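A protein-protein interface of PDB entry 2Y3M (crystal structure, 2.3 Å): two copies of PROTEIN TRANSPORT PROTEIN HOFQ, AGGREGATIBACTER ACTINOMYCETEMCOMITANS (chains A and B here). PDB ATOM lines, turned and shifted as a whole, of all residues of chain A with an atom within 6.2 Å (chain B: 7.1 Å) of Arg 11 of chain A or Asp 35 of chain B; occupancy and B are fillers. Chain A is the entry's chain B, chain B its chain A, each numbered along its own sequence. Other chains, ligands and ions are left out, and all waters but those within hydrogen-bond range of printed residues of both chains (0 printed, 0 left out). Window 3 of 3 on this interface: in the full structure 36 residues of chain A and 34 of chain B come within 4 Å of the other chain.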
ATOM      1  N   SER A   9      27.397  29.110   8.940  1.00  0.00           N
ATOM      2  CA  SER A   9      26.104  28.450   9.000  1.00  0.00           C
ATOM      3  C   SER A   9      25.729  28.167  10.440  1.00  0.00           C
ATOM      4  O   SER A   9      26.559  27.712  11.223  1.00  0.00           O
ATOM      5  CB  SER A   9      26.144  27.142   8.220  1.00  0.00           C
ATOM      6  OG  SER A   9      24.837  26.716   7.908  1.00  0.00           O
ATOM      7  N   ILE A  10      24.477  28.447  10.788  1.00  0.00           N
ATOM      8  CA  ILE A  10      23.976  28.149  12.124  1.00  0.00           C
ATOM      9  C   ILE A  10      22.535  27.628  12.080  1.00  0.00           C
ATOM     10  O   ILE A  10      21.688  28.133  11.336  1.00  0.00           O
ATOM     11  CB  ILE A  10      24.136  29.363  13.084  1.00  0.00           C
ATOM     12  CG1 ILE A  10      23.763  28.977  14.525  1.00  0.00           C
ATOM     13  CG2 ILE A  10      23.351  30.569  12.571  1.00  0.00           C
ATOM     14  CD1 ILE A  10      24.077  30.044  15.560  1.00  0.00           C
ATOM     15  N   ARG A  11      22.286  26.586  12.863  1.00  0.00           N
ATOM     16  CA  ARG A  11      20.969  25.983  12.955  1.00  0.00           C
ATOM     17  C   ARG A  11      20.244  26.498  14.196  1.00  0.00           C
ATOM     18  O   ARG A  11      20.793  26.487  15.298  1.00  0.00           O
ATOM     19  CB  ARG A  11      21.092  24.457  12.965  1.00  0.00           C
ATOM     20  CG  ARG A  11      19.768  23.706  12.988  1.00  0.00           C
ATOM     21  CD  ARG A  11      19.973  22.235  12.644  1.00  0.00           C
ATOM     22  NE  ARG A  11      20.282  22.053  11.226  1.00  0.00           N
ATOM     23  CZ  ARG A  11      19.394  21.690  10.303  1.00  0.00           C
ATOM     24  NH1 ARG A  11      18.131  21.458  10.642  1.00  0.00           N
ATOM     25  NH2 ARG A  11      19.768  21.551   9.040  1.00  0.00           N
ATOM     26  N   LEU A  12      19.021  26.978  13.996  1.00  0.00           N
ATOM     27  CA  LEU A  12      18.146  27.375  15.094  1.00  0.00           C
ATOM     28  C   LEU A  12      17.032  26.348  15.240  1.00  0.00           C
ATOM     29  O   LEU A  12      16.246  26.134  14.315  1.00  0.00           O
ATOM     30  CB  LEU A  12      17.549  28.774  14.862  1.00  0.00           C
ATOM     31  CG  LEU A  12      18.443  30.018  14.719  1.00  0.00           C
ATOM     32  CD1 LEU A  12      17.584  31.279  14.665  1.00  0.00           C
ATOM     33  CD2 LEU A  12      19.454  30.126  15.849  1.00  0.00           C
ATOM     34  N   LYS A  13      16.986  25.700  16.397  1.00  0.00           N
ATOM     35  CA  LYS A  13      15.940  24.730  16.707  1.00  0.00           C
ATOM     36  C   LYS A  13      14.917  25.386  17.632  1.00  0.00           C
ATOM     37  O   LYS A  13      15.291  26.185  18.495  1.00  0.00           O
ATOM     38  CB  LYS A  13      16.549  23.485  17.368  1.00  0.00           C
ATOM     39  CG  LYS A  13      15.666  22.236  17.300  1.00  0.00           C
ATOM     40  CD  LYS A  13      16.265  21.047  18.050  1.00  0.00           C
ATOM     41  CE  LYS A  13      17.282  20.284  17.198  1.00  0.00           C
ATOM     42  NZ  LYS A  13      17.593  18.927  17.748  1.00  0.00           N
ATOM     43  N   GLN A  68      16.880  27.805  20.278  1.00  0.00           N
ATOM     44  CA  GLN A  68      18.187  27.366  20.745  1.00  0.00           C
ATOM     45  C   GLN A  68      19.131  27.197  19.563  1.00  0.00           C
ATOM     46  O   GLN A  68      18.741  26.727  18.491  1.00  0.00           O
ATOM     47  CB  GLN A  68      18.100  26.093  21.596  1.00  0.00           C
ATOM     48  CG  GLN A  68      17.257  24.963  21.015  1.00  0.00           C
ATOM     49  CD  GLN A  68      16.753  24.002  22.089  1.00  0.00           C
ATOM     50  OE1 GLN A  68      16.478  24.402  23.224  1.00  0.00           O
ATOM     51  NE2 GLN A  68      16.626  22.729  21.729  1.00  0.00           N
ATOM     52  N   GLU A  69      20.371  27.617  19.762  1.00  0.00           N
ATOM     53  CA  GLU A  69      21.357  27.595  18.696  1.00  0.00           C
ATOM     54  C   GLU A  69      22.450  26.570  18.957  1.00  0.00           C
ATOM     55  O   GLU A  69      22.985  26.473  20.065  1.00  0.00           O
ATOM     56  CB  GLU A  69      21.948  28.992  18.454  1.00  0.00           C
ATOM     57  CG  GLU A  69      22.036  29.894  19.685  1.00  0.00           C
ATOM     58  CD  GLU A  69      22.805  31.184  19.428  1.00  0.00           C
ATOM     59  OE1 GLU A  69      23.772  31.170  18.637  1.00  0.00           O
ATOM     60  OE2 GLU A  69      22.449  32.215  20.035  1.00  0.00           O
ATOM     61  N   ASN A  70      22.749  25.790  17.923  1.00  0.00           N
ATOM     62  CA  ASN A  70      23.864  24.862  17.936  1.00  0.00           C
ATOM     63  C   ASN A  70      25.119  25.603  17.473  1.00  0.00           C
ATOM     64  O   ASN A  70      25.050  26.791  17.154  1.00  0.00           O
ATOM     65  CB  ASN A  70      23.548  23.660  17.041  1.00  0.00           C
ATOM     66  CG  ASN A  70      22.352  22.852  17.545  1.00  0.00           C
ATOM     67  OD1 ASN A  70      21.402  22.595  16.802  1.00  0.00           O
ATOM     68  ND2 ASN A  70      22.391  22.462  18.820  1.00  0.00           N
ATOM     69  N   GLY A  71      26.261  24.924  17.449  1.00  0.00           N
ATOM     70  CA  GLY A  71      27.505  25.556  17.010  1.00  0.00           C
ATOM     71  C   GLY A  71      27.429  26.131  15.604  1.00  0.00           C
ATOM     72  O   GLY A  71      26.586  25.726  14.800  1.00  0.00           O
ATOM     73  N   ILE B  33      16.942  28.556   5.318  1.00  0.00           N
ATOM     74  CA  ILE B  33      16.350  27.272   4.924  1.00  0.00           C
ATOM     75  C   ILE B  33      15.527  26.692   6.074  1.00  0.00           C
ATOM     76  O   ILE B  33      15.999  26.622   7.211  1.00  0.00           O
ATOM     77  CB  ILE B  33      17.422  26.229   4.497  1.00  0.00           C
ATOM     78  CG1 ILE B  33      18.270  26.753   3.331  1.00  0.00           C
ATOM     79  CG2 ILE B  33      16.764  24.897   4.126  1.00  0.00           C
ATOM     80  CD1 ILE B  33      19.573  25.983   3.101  1.00  0.00           C
ATOM     81  N   ILE B  34      14.305  26.265   5.765  1.00  0.00           N
ATOM     82  CA  ILE B  34      13.397  25.710   6.768  1.00  0.00           C
ATOM     83  C   ILE B  34      13.332  24.187   6.648  1.00  0.00           C
ATOM     84  O   ILE B  34      13.140  23.654   5.553  1.00  0.00           O
ATOM     85  CB  ILE B  34      11.971  26.329   6.652  1.00  0.00           C
ATOM     86  CG1 ILE B  34      12.001  27.841   6.908  1.00  0.00           C
ATOM     87  CG2 ILE B  34      10.996  25.676   7.631  1.00  0.00           C
ATOM     88  CD1 ILE B  34      12.302  28.702   5.675  1.00  0.00           C
ATOM     89  N   ASP B  35      13.509  23.500   7.777  1.00  0.00           N
ATOM     90  CA  ASP B  35      13.286  22.055   7.857  1.00  0.00           C
ATOM     91  C   ASP B  35      11.932  21.770   8.492  1.00  0.00           C
ATOM     92  O   ASP B  35      11.638  22.258   9.583  1.00  0.00           O
ATOM     93  CB  ASP B  35      14.392  21.365   8.665  1.00  0.00           C
ATOM     94  CG  ASP B  35      15.723  21.305   7.923  1.00  0.00           C
ATOM     95  OD1 ASP B  35      15.856  21.931   6.836  1.00  0.00           O
ATOM     96  OD2 ASP B  35      16.646  20.621   8.437  1.00  0.00           O
ATOM     97  N   THR B  41       8.421  19.258  14.788  1.00  0.00           N
ATOM     98  CA  THR B  41       8.925  20.593  15.108  1.00  0.00           C
ATOM     99  C   THR B  41       9.692  21.188  13.922  1.00  0.00           C
ATOM    100  O   THR B  41       9.884  20.521  12.901  1.00  0.00           O
ATOM    101  CB  THR B  41       9.832  20.582  16.365  1.00  0.00           C
ATOM    102  OG1 THR B  41      11.098  19.987  16.046  1.00  0.00           O
ATOM    103  CG2 THR B  41       9.173  19.809  17.515  1.00  0.00           C
ATOM    104  N   VAL B  42      10.136  22.434  14.064  1.00  0.00           N
ATOM    105  CA  VAL B  42      10.791  23.150  12.971  1.00  0.00           C
ATOM    106  C   VAL B  42      12.226  23.558  13.312  1.00  0.00           C
ATOM    107  O   VAL B  42      12.538  23.866  14.466  1.00  0.00           O
ATOM    108  CB  VAL B  42       9.948  24.386  12.516  1.00  0.00           C
ATOM    109  CG1 VAL B  42       9.557  25.260  13.711  1.00  0.00           C
ATOM    110  CG2 VAL B  42      10.674  25.203  11.444  1.00  0.00           C
ATOM    111  N   SER B  43      13.084  23.531  12.291  1.00  0.00           N
ATOM    112  CA  SER B  43      14.447  24.051  12.365  1.00  0.00           C
ATOM    113  C   SER B  43      14.694  25.078  11.264  1.00  0.00           C
ATOM    114  O   SER B  43      14.170  24.948  10.156  1.00  0.00           O
ATOM    115  CB  SER B  43      15.467  22.922  12.234  1.00  0.00           C
ATOM    116  OG  SER B  43      15.523  22.158  13.419  1.00  0.00           O
ATOM    117  N   LEU B  44      15.495  26.091  11.582  1.00  0.00           N
ATOM    118  CA  LEU B  44      15.914  27.088  10.604  1.00  0.00           C
ATOM    119  C   LEU B  44      17.422  27.014  10.419  1.00  0.00           C
ATOM    120  O   LEU B  44      18.171  27.004  11.392  1.00  0.00           O
ATOM    121  CB  LEU B  44      15.532  28.504  11.051  1.00  0.00           C
ATOM    122  CG  LEU B  44      14.128  28.840  11.563  1.00  0.00           C
ATOM    123  CD1 LEU B  44      14.071  30.314  11.949  1.00  0.00           C
ATOM    124  CD2 LEU B  44      13.045  28.504  10.536  1.00  0.00           C
ATOM    125  N   GLN B  45      17.864  26.964   9.170  1.00  0.00           N
ATOM    126  CA  GLN B  45      19.284  26.995   8.873  1.00  0.00           C
ATOM    127  C   GLN B  45      19.622  28.326   8.222  1.00  0.00           C
ATOM    128  O   GLN B  45      19.035  28.684   7.208  1.00  0.00           O
ATOM    129  CB  GLN B  45      19.675  25.826   7.976  1.00  0.00           C
ATOM    130  CG  GLN B  45      21.163  25.551   7.960  1.00  0.00           C
ATOM    131  CD  GLN B  45      21.520  24.286   7.207  1.00  0.00           C
ATOM    132  OE1 GLN B  45      20.836  23.268   7.317  1.00  0.00           O
ATOM    133  NE2 GLN B  45      22.605  24.343   6.442  1.00  0.00           N
ATOM    134  N   LEU B  46      20.552  29.057   8.827  1.00  0.00           N
ATOM    135  CA  LEU B  46      20.944  30.383   8.359  1.00  0.00           C
ATOM    136  C   LEU B  46      22.370  30.369   7.835  1.00  0.00           C
ATOM    137  O   LEU B  46      23.265  29.807   8.468  1.00  0.00           O
ATOM    138  CB  LEU B  46      20.846  31.418   9.486  1.00  0.00           C
ATOM    139  CG  LEU B  46      19.515  31.759  10.160  1.00  0.00           C
ATOM    140  CD1 LEU B  46      19.778  32.757  11.263  1.00  0.00           C
ATOM    141  CD2 LEU B  46      18.503  32.329   9.179  1.00  0.00           C
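Ser 9 of chain A touches Gln 45 of chain B (OG to NE2, 3.6 Å). Ser 9 of chain A touches Leu 46 of chain B (CA to O, 3.2 Å). Leu 44 of chain B touches Ile 10 of chain A (O to O, 3.7 Å). Gln 45 of chain B touches Ile 10 of chain A (CA to O, 3.6 Å). Ser 43 of chain B touches Arg 11 of chain A (CB to NH1, 3.4 Å). Leu 44 of chain B touches Arg 11 of chain A (O to CA, 3.4 Å). Leu 12 of chain A touches Ser 43 of chain B (O to CA, 3.4 Å). Lys 13 of chain A touches Ser 43 of chain B (CG to OG, 3.9 Å).
Asp 35 of chain B touches just one residue of chain A: Arg 11. Printed residues of chain B within 4 Å of Ile 10 of chain A: Leu 44 (3.7 Å), Gln 45 (3.6 Å) and Leu 46 (2.9 Å). Of the printed residues of chain A, Gln 45 of chain B touches Ser 9 (3.6 Å), Ile 10 (3.6 Å) and Arg 11 (2.7 Å). Gly 71 of chain A touches none of the printed residues of chain B. The nearest residue of chain B that does not touch Arg 11 of chain A is Leu 46 of chain B (5.0 Å). The nearest printed residue of chain B that does not touch Ile 10 of chain A is Ile 33 of chain B (7.2 Å).
The side-chain carboxylate (OD2) of Asp 35 of chain B is in salt-bridge range of the guanidinium group (NH1) of Arg 11 of chain A (2.8 Å). The backbone carbonyl oxygen (O) of Leu 44 of chain B lies within hydrogen-bond range of the backbone NH (N) of Leu 12 of chain A (2.7 Å). The side-chain amide oxygen (OE1) of Gln 45 of chain B sits at hydrogen-bond distance from the guanidinium group (NH2) of Arg 11 of chain A (2.7 Å). The backbone carbonyl oxygen (O) of Ile 10 of chain A sits at hydrogen-bond distance from the backbone NH (N) of Leu 46 of chain B (2.9 Å).
Among the printed residues, 12 pairs touch across the chains. Among the printed residues, Asp or Glu carboxylates within 4 Å of a Lys or Arg side-chain nitrogen of the other chain: Arg 11 of chain A with Asp 35 of chain B.
No position is printed for both chains. Of the 12 pairs that touch across the chains among the printed residues, none has its exchanged pair printed and touching as well.
The backbone carbonyl oxygen (O) of Ile 33 of chain B sits at hydrogen-bond distance from the backbone NH (N) of Gln 45 of chain B. The backbone NH of Asp 35 of chain B is in hydrogen-bond range of the backbone carbonyl oxygen of Ser 43 of chain B (2.9 Å). The backbone carbonyl oxygen (O) of Arg 11 of chain A is in hydrogen-bond range of the backbone NH (N) of Asn 70 of chain A (3.3 Å). The backbone carbonyl oxygen of Lys 13 of chain A sits at hydrogen-bond distance from the backbone NH of Gln 68 of chain A.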
